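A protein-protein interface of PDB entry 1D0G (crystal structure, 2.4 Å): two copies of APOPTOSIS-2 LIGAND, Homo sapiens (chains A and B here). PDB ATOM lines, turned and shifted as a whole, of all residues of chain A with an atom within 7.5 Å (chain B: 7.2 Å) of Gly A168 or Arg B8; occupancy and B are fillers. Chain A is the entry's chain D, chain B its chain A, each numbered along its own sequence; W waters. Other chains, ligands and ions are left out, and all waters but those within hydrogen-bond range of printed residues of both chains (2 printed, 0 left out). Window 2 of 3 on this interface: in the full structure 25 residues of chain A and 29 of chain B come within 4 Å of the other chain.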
ATOM      1  N   LYS A  66     -29.037   3.723  18.635  1.00  0.00           N
ATOM      2  CA  LYS A  66     -29.529   3.454  19.962  1.00  0.00           C
ATOM      3  C   LYS A  66     -29.608   1.936  20.156  1.00  0.00           C
ATOM      4  O   LYS A  66     -29.768   1.177  19.199  1.00  0.00           O
ATOM      5  CB  LYS A  66     -30.875   4.119  20.178  1.00  0.00           C
ATOM      6  CG  LYS A  66     -32.055   3.241  19.978  1.00  0.00           C
ATOM      7  CD  LYS A  66     -33.282   3.977  20.434  1.00  0.00           C
ATOM      8  CE  LYS A  66     -34.490   3.063  20.450  1.00  0.00           C
ATOM      9  NZ  LYS A  66     -35.737   3.829  20.738  1.00  0.00           N
ATOM     10  N   GLY A  67     -29.386   1.504  21.391  1.00  0.00           N
ATOM     11  CA  GLY A  67     -29.419   0.092  21.687  1.00  0.00           C
ATOM     12  C   GLY A  67     -28.662  -0.278  22.940  1.00  0.00           C
ATOM     13  O   GLY A  67     -28.264   0.569  23.745  1.00  0.00           O
ATOM     14  N   PHE A  68     -28.531  -1.577  23.126  1.00  0.00           N
ATOM     15  CA  PHE A  68     -27.813  -2.120  24.252  1.00  0.00           C
ATOM     16  C   PHE A  68     -26.319  -2.167  23.905  1.00  0.00           C
ATOM     17  O   PHE A  68     -25.925  -2.740  22.893  1.00  0.00           O
ATOM     18  CB  PHE A  68     -28.339  -3.525  24.572  1.00  0.00           C
ATOM     19  CG  PHE A  68     -29.747  -3.549  25.120  1.00  0.00           C
ATOM     20  CD1 PHE A  68     -30.213  -2.526  25.953  1.00  0.00           C
ATOM     21  CD2 PHE A  68     -30.606  -4.598  24.810  1.00  0.00           C
ATOM     22  CE1 PHE A  68     -31.511  -2.549  26.472  1.00  0.00           C
ATOM     23  CE2 PHE A  68     -31.908  -4.635  25.321  1.00  0.00           C
ATOM     24  CZ  PHE A  68     -32.362  -3.602  26.156  1.00  0.00           C
ATOM     25  N   TYR A  69     -25.503  -1.522  24.733  1.00  0.00           N
ATOM     26  CA  TYR A  69     -24.054  -1.513  24.525  1.00  0.00           C
ATOM     27  C   TYR A  69     -23.273  -2.040  25.703  1.00  0.00           C
ATOM     28  O   TYR A  69     -23.511  -1.646  26.845  1.00  0.00           O
ATOM     29  CB  TYR A  69     -23.533  -0.114  24.252  1.00  0.00           C
ATOM     30  CG  TYR A  69     -23.851   0.419  22.900  1.00  0.00           C
ATOM     31  CD1 TYR A  69     -25.105   0.988  22.623  1.00  0.00           C
ATOM     32  CD2 TYR A  69     -22.890   0.386  21.889  1.00  0.00           C
ATOM     33  CE1 TYR A  69     -25.394   1.505  21.359  1.00  0.00           C
ATOM     34  CE2 TYR A  69     -23.159   0.907  20.621  1.00  0.00           C
ATOM     35  CZ  TYR A  69     -24.411   1.460  20.361  1.00  0.00           C
ATOM     36  OH  TYR A  69     -24.667   1.959  19.108  1.00  0.00           O
ATOM     37  N   ILE A 134     -23.490  -3.753  30.442  1.00  0.00           N
ATOM     38  CA  ILE A 134     -24.403  -3.403  29.363  1.00  0.00           C
ATOM     39  C   ILE A 134     -25.347  -2.289  29.807  1.00  0.00           C
ATOM     40  O   ILE A 134     -26.033  -2.417  30.827  1.00  0.00           O
ATOM     41  CB  ILE A 134     -25.331  -4.579  28.991  1.00  0.00           C
ATOM     42  CG1 ILE A 134     -24.547  -5.872  28.780  1.00  0.00           C
ATOM     43  CG2 ILE A 134     -26.144  -4.234  27.736  1.00  0.00           C
ATOM     44  CD1 ILE A 134     -25.466  -7.082  28.876  1.00  0.00           C
ATOM     45  N   GLU A 136     -28.305   0.753  28.130  1.00  0.00           N
ATOM     46  CA  GLU A 136     -29.085   1.222  26.977  1.00  0.00           C
ATOM     47  C   GLU A 136     -28.723   2.687  26.673  1.00  0.00           C
ATOM     48  O   GLU A 136     -28.826   3.562  27.528  1.00  0.00           O
ATOM     49  CB  GLU A 136     -30.576   1.043  27.238  1.00  0.00           C
ATOM     50  CG  GLU A 136     -31.490   1.337  26.052  1.00  0.00           C
ATOM     51  CD  GLU A 136     -32.964   1.061  26.382  1.00  0.00           C
ATOM     52  OE1 GLU A 136     -33.398   1.387  27.517  1.00  0.00           O
ATOM     53  OE2 GLU A 136     -33.677   0.492  25.521  1.00  0.00           O
ATOM     54  N   LEU A 137     -28.265   2.921  25.447  1.00  0.00           N
ATOM     55  CA  LEU A 137     -27.838   4.256  25.022  1.00  0.00           C
ATOM     56  C   LEU A 137     -28.640   4.787  23.837  1.00  0.00           C
ATOM     57  O   LEU A 137     -28.889   4.058  22.868  1.00  0.00           O
ATOM     58  CB  LEU A 137     -26.363   4.218  24.644  1.00  0.00           C
ATOM     59  CG  LEU A 137     -25.385   3.782  25.726  1.00  0.00           C
ATOM     60  CD1 LEU A 137     -23.970   3.780  25.160  1.00  0.00           C
ATOM     61  CD2 LEU A 137     -25.491   4.735  26.913  1.00  0.00           C
ATOM     62  N   PHE A 165     -19.616  -2.039  22.292  1.00  0.00           N
ATOM     63  CA  PHE A 165     -20.212  -2.736  21.148  1.00  0.00           C
ATOM     64  C   PHE A 165     -21.683  -3.020  21.375  1.00  0.00           C
ATOM     65  O   PHE A 165     -22.125  -3.214  22.504  1.00  0.00           O
ATOM     66  CB  PHE A 165     -19.455  -4.022  20.752  1.00  0.00           C
ATOM     67  CG  PHE A 165     -19.373  -5.067  21.829  1.00  0.00           C
ATOM     68  CD1 PHE A 165     -20.356  -6.028  21.958  1.00  0.00           C
ATOM     69  CD2 PHE A 165     -18.265  -5.143  22.656  1.00  0.00           C
ATOM     70  CE1 PHE A 165     -20.235  -7.046  22.886  1.00  0.00           C
ATOM     71  CE2 PHE A 165     -18.138  -6.171  23.590  1.00  0.00           C
ATOM     72  CZ  PHE A 165     -19.120  -7.115  23.700  1.00  0.00           C
ATOM     73  N   LEU A 166     -22.446  -2.979  20.298  1.00  0.00           N
ATOM     74  CA  LEU A 166     -23.880  -3.228  20.366  1.00  0.00           C
ATOM     75  C   LEU A 166     -24.091  -4.701  20.703  1.00  0.00           C
ATOM     76  O   LEU A 166     -23.503  -5.575  20.060  1.00  0.00           O
ATOM     77  CB  LEU A 166     -24.482  -2.867  19.014  1.00  0.00           C
ATOM     78  CG  LEU A 166     -25.946  -2.511  18.852  1.00  0.00           C
ATOM     79  CD1 LEU A 166     -26.448  -1.616  19.934  1.00  0.00           C
ATOM     80  CD2 LEU A 166     -26.038  -1.776  17.547  1.00  0.00           C
ATOM     81  N   VAL A 167     -24.849  -4.964  21.755  1.00  0.00           N
ATOM     82  CA  VAL A 167     -25.083  -6.327  22.183  1.00  0.00           C
ATOM     83  C   VAL A 167     -26.498  -6.917  22.061  1.00  0.00           C
ATOM     84  O   VAL A 167     -26.940  -7.511  23.009  1.00  0.00           O
ATOM     85  CB  VAL A 167     -24.622  -6.568  23.692  1.00  0.00           C
ATOM     86  CG1 VAL A 167     -23.127  -6.412  23.885  1.00  0.00           C
ATOM     87  CG2 VAL A 167     -25.340  -5.615  24.628  1.00  0.00           C
ATOM     88  N   GLY A 168     -27.212  -6.813  20.940  1.00  0.00           N
ATOM     89  CA  GLY A 168     -28.543  -7.446  20.847  1.00  0.00           C
ATOM     90  C   GLY A 168     -28.729  -8.974  20.659  1.00  0.00           C
ATOM     91  O   GLY A 168     -28.584  -9.569  19.562  1.00  0.00           O
ATOM     92  OXT GLY A 168     -29.134  -9.607  21.643  1.00  0.00           O
ATOM     93  N   PRO B   6     -36.895  -6.045  21.280  1.00  0.00           N
ATOM     94  CA  PRO B   6     -38.002  -7.037  21.349  1.00  0.00           C
ATOM     95  C   PRO B   6     -37.515  -8.491  21.213  1.00  0.00           C
ATOM     96  O   PRO B   6     -38.124  -9.424  21.770  1.00  0.00           O
ATOM     97  N   GLN B   7     -36.441  -8.665  20.440  1.00  0.00           N
ATOM     98  CA  GLN B   7     -35.840  -9.973  20.187  1.00  0.00           C
ATOM     99  C   GLN B   7     -34.397 -10.006  20.677  1.00  0.00           C
ATOM    100  O   GLN B   7     -33.619 -10.897  20.320  1.00  0.00           O
ATOM    101  CB  GLN B   7     -35.891 -10.307  18.693  1.00  0.00           C
ATOM    102  CG  GLN B   7     -37.280 -10.685  18.187  1.00  0.00           C
ATOM    103  CD  GLN B   7     -37.832 -11.954  18.838  1.00  0.00           C
ATOM    104  OE1 GLN B   7     -37.121 -12.953  18.995  1.00  0.00           O
ATOM    105  NE2 GLN B   7     -39.108 -11.924  19.204  1.00  0.00           N
ATOM    106  N   ARG B   8     -34.039  -9.002  21.471  1.00  0.00           N
ATOM    107  CA  ARG B   8     -32.704  -8.905  22.046  1.00  0.00           C
ATOM    108  C   ARG B   8     -32.691  -9.694  23.352  1.00  0.00           C
ATOM    109  O   ARG B   8     -33.643  -9.623  24.134  1.00  0.00           O
ATOM    110  CB  ARG B   8     -32.343  -7.436  22.283  1.00  0.00           C
ATOM    111  CG  ARG B   8     -32.234  -6.643  20.997  1.00  0.00           C
ATOM    112  CD  ARG B   8     -33.178  -5.461  20.992  1.00  0.00           C
ATOM    113  NE  ARG B   8     -32.529  -4.296  21.591  1.00  0.00           N
ATOM    114  CZ  ARG B   8     -33.136  -3.394  22.360  1.00  0.00           C
ATOM    115  NH1 ARG B   8     -34.425  -3.502  22.643  1.00  0.00           N
ATOM    116  NH2 ARG B   8     -32.447  -2.369  22.843  1.00  0.00           N
ATOM    117  N   VAL B   9     -31.644 -10.485  23.565  1.00  0.00           N
ATOM    118  CA  VAL B   9     -31.555 -11.272  24.798  1.00  0.00           C
ATOM    119  C   VAL B   9     -30.377 -10.813  25.677  1.00  0.00           C
ATOM    120  O   VAL B   9     -29.245 -11.267  25.504  1.00  0.00           O
ATOM    121  CB  VAL B   9     -31.405 -12.772  24.512  1.00  0.00           C
ATOM    122  CG1 VAL B   9     -31.760 -13.547  25.734  1.00  0.00           C
ATOM    123  CG2 VAL B   9     -32.296 -13.195  23.345  1.00  0.00           C
ATOM    124  N   ALA B  10     -30.651  -9.930  26.635  1.00  0.00           N
ATOM    125  CA  ALA B  10     -29.611  -9.405  27.508  1.00  0.00           C
ATOM    126  C   ALA B  10     -30.235  -8.913  28.808  1.00  0.00           C
ATOM    127  O   ALA B  10     -31.462  -8.784  28.903  1.00  0.00           O
ATOM    128  CB  ALA B  10     -28.861  -8.275  26.809  1.00  0.00           C
ATOM    129  N   ALA B  11     -29.389  -8.643  29.801  1.00  0.00           N
ATOM    130  CA  ALA B  11     -29.843  -8.168  31.093  1.00  0.00           C
ATOM    131  C   ALA B  11     -28.686  -7.567  31.857  1.00  0.00           C
ATOM    132  O   ALA B  11     -27.559  -8.049  31.777  1.00  0.00           O
ATOM    133  CB  ALA B  11     -30.457  -9.336  31.920  1.00  0.00           C
ATOM    134  N   PHE B  50     -32.141  -3.479  33.518  1.00  0.00           N
ATOM    135  CA  PHE B  50     -33.175  -3.945  32.618  1.00  0.00           C
ATOM    136  C   PHE B  50     -33.080  -5.451  32.458  1.00  0.00           C
ATOM    137  O   PHE B  50     -32.032  -6.061  32.696  1.00  0.00           O
ATOM    138  CB  PHE B  50     -33.023  -3.298  31.247  1.00  0.00           C
ATOM    139  CG  PHE B  50     -31.854  -3.813  30.464  1.00  0.00           C
ATOM    140  CD1 PHE B  50     -31.993  -4.931  29.632  1.00  0.00           C
ATOM    141  CD2 PHE B  50     -30.602  -3.216  30.576  1.00  0.00           C
ATOM    142  CE1 PHE B  50     -30.898  -5.450  28.925  1.00  0.00           C
ATOM    143  CE2 PHE B  50     -29.505  -3.725  29.875  1.00  0.00           C
ATOM    144  CZ  PHE B  50     -29.651  -4.845  29.050  1.00  0.00           C
ATOM    145  N   LEU B  51     -34.174  -6.029  31.985  1.00  0.00           N
ATOM    146  CA  LEU B  51     -34.288  -7.449  31.724  1.00  0.00           C
ATOM    147  C   LEU B  51     -34.900  -7.531  30.340  1.00  0.00           C
ATOM    148  O   LEU B  51     -35.906  -6.892  30.097  1.00  0.00           O
ATOM    149  CB  LEU B  51     -35.232  -8.075  32.745  1.00  0.00           C
ATOM    150  CG  LEU B  51     -34.650  -8.222  34.147  1.00  0.00           C
ATOM    151  CD1 LEU B  51     -35.758  -8.540  35.129  1.00  0.00           C
ATOM    152  CD2 LEU B  51     -33.611  -9.328  34.119  1.00  0.00           C
ATOM    153  N   SER B  52     -34.261  -8.250  29.422  1.00  0.00           N
ATOM    154  CA  SER B  52     -34.775  -8.423  28.045  1.00  0.00           C
ATOM    155  C   SER B  52     -34.678  -9.912  27.598  1.00  0.00           C
ATOM    156  O   SER B  52     -33.623 -10.377  27.151  1.00  0.00           O
ATOM    157  CB  SER B  52     -34.015  -7.505  27.091  1.00  0.00           C
ATOM    158  OG  SER B  52     -34.375  -7.740  25.745  1.00  0.00           O
ATOM    159  N   ASN B  53     -35.773 -10.649  27.789  1.00  0.00           N
ATOM    160  CA  ASN B  53     -35.883 -12.073  27.462  1.00  0.00           C
ATOM    161  C   ASN B  53     -35.216 -12.973  28.490  1.00  0.00           C
ATOM    162  O   ASN B  53     -34.641 -14.015  28.180  1.00  0.00           O
ATOM    163  CB  ASN B  53     -35.399 -12.358  26.041  1.00  0.00           C
ATOM    164  CG  ASN B  53     -36.451 -12.012  25.010  1.00  0.00           C
ATOM    165  OD1 ASN B  53     -37.554 -12.555  25.043  1.00  0.00           O
ATOM    166  ND2 ASN B  53     -36.131 -11.089  24.110  1.00  0.00           N
ATOM    167  N   LEU B  54     -35.288 -12.506  29.724  1.00  0.00           N
ATOM    168  CA  LEU B  54     -34.766 -13.177  30.897  1.00  0.00           C
ATOM    169  C   LEU B  54     -35.569 -12.522  32.008  1.00  0.00           C
ATOM    170  O   LEU B  54     -36.208 -11.477  31.798  1.00  0.00           O
ATOM    171  CB  LEU B  54     -33.283 -12.855  31.144  1.00  0.00           C
ATOM    172  CG  LEU B  54     -32.078 -13.487  30.447  1.00  0.00           C
ATOM    173  CD1 LEU B  54     -31.714 -12.713  29.197  1.00  0.00           C
ATOM    174  CD2 LEU B  54     -30.913 -13.423  31.413  1.00  0.00           C
ATOM    175  N   PHE B 165     -25.628 -11.692  28.311  1.00  0.00           N
ATOM    176  CA  PHE B 165     -26.145 -11.454  26.989  1.00  0.00           C
ATOM    177  C   PHE B 165     -25.786 -12.597  26.057  1.00  0.00           C
ATOM    178  O   PHE B 165     -24.767 -13.259  26.223  1.00  0.00           O
ATOM    179  CB  PHE B 165     -25.723 -10.076  26.426  1.00  0.00           C
ATOM    180  CG  PHE B 165     -24.240  -9.875  26.286  1.00  0.00           C
ATOM    181  CD1 PHE B 165     -23.569 -10.294  25.153  1.00  0.00           C
ATOM    182  CD2 PHE B 165     -23.518  -9.157  27.256  1.00  0.00           C
ATOM    183  CE1 PHE B 165     -22.203 -10.000  24.979  1.00  0.00           C
ATOM    184  CE2 PHE B 165     -22.167  -8.865  27.090  1.00  0.00           C
ATOM    185  CZ  PHE B 165     -21.515  -9.287  25.943  1.00  0.00           C
ATOM    186  N   LEU B 166     -26.683 -12.865  25.114  1.00  0.00           N
ATOM    187  CA  LEU B 166     -26.508 -13.927  24.143  1.00  0.00           C
ATOM    188  C   LEU B 166     -25.389 -13.515  23.213  1.00  0.00           C
ATOM    189  O   LEU B 166     -25.412 -12.410  22.649  1.00  0.00           O
ATOM    190  CB  LEU B 166     -27.804 -14.120  23.364  1.00  0.00           C
ATOM    191  CG  LEU B 166     -28.092 -15.475  22.726  1.00  0.00           C
ATOM    192  CD1 LEU B 166     -27.932 -16.628  23.713  1.00  0.00           C
ATOM    193  CD2 LEU B 166     -29.523 -15.405  22.236  1.00  0.00           C
ATOM    194  N   VAL B 167     -24.354 -14.346  23.156  1.00  0.00           N
ATOM    195  CA  VAL B 167     -23.208 -14.095  22.290  1.00  0.00           C
ATOM    196  C   VAL B 167     -23.382 -15.142  21.219  1.00  0.00           C
ATOM    197  O   VAL B 167     -23.890 -16.213  21.484  1.00  0.00           O
ATOM    198  CB  VAL B 167     -21.856 -14.309  22.994  1.00  0.00           C
ATOM    199  CG1 VAL B 167     -21.643 -13.252  23.987  1.00  0.00           C
ATOM    200  CG2 VAL B 167     -21.770 -15.665  23.624  1.00  0.00           C
HETATM  201  O   HOH W   1     -32.611   0.094  23.296  1.00  0.00           O
HETATM  202  O   HOH W   2     -29.723  -3.672  21.016  1.00  0.00           O
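The backbone NH (N) of Val B9 sits at hydrogen-bond distance from the chain-end carboxylate (OXT) of Gly A168 (3.3 Å).
The backbone carbonyl oxygen (O) of Arg B8 sits at hydrogen-bond distance from the side-chain hydroxyl (OG) of Ser B52, 2.6 Å away.
The backbone carbonyl oxygen (O) of Arg B8 is in hydrogen-bond range of the side-chain amide nitrogen (ND2) of Asn B53 (2.9 Å).
The backbone NH (N) of Leu B166 sits at hydrogen-bond distance from the backbone carbonyl oxygen (O) of Val B9.
The backbone carbonyl oxygen (O) of Ala B10 is in hydrogen-bond range of the backbone NH (N) of Ser B52, 2.9 Å away.
The backbone carbonyl oxygen of Phe A68 is in hydrogen-bond range of the backbone NH of Val A167 (2.7 Å).
Among the printed residues, merely in contact across the chains: Ile A134 with Phe B165, Phe A68 with Arg B8, Phe A68 with Phe B50, Gly A168 with Arg B8, Ile A134 with Ala B11, Ile A134 with Phe B50, Val A167 with Phe B165, Phe A165 with Phe B165 and Phe A68 with Ser B52.
Of chain B, only Arg B8 (3.7 Å) and Val B9 (3.3 Å) come within 4 Å of Gly A168.
Printed residues of chain A within 4 Å of Ala B11: Ile A134.
Printed residues of chain A within 4 Å of Ser B52: Phe A68.
Printed residues of chain A within 4 Å of Val B9: Gly A168.
Of the printed residues of chain B, Phe A165 touches Phe B165 (3.9 Å).
The nearest residue of chain B that does not touch Gly A168 is Leu B166 (4.8 Å).
Of the 14 printed residues of chain B, 6 touch a printed residue of chain A.
Printed residues of chain B that touch a printed residue of chain A: Arg B8, Val B9, Ala B11, Phe B50, Ser B52 and Phe B165.
Of the 11 printed residues of chain A, 5 touch a printed residue of chain B.
Hydrophobic or aromatic side chains of chain A within 4 Å of the printed part of chain B: Phe A68, Ile A134, Phe A165 and Val A167.
Among the printed residues, no Asp or Glu carboxylate lies within 4 Å of a Lys or Arg side-chain nitrogen of the other chain.
Phe B165 touches its own counterpart, Phe A165.
Val A167 touches Phe B165, but with the chains exchanged Phe A165 does not touch Val B167 (6.5 Å).
Water W1 bridges OE2 of Glu A136 (2.5 Å) and NH2 of Arg B8 (2.5 Å).
Water W2 lies within hydrogen-bond range of NE of Arg B8 (2.9 Å) and N of Phe A68 (3.2 Å).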
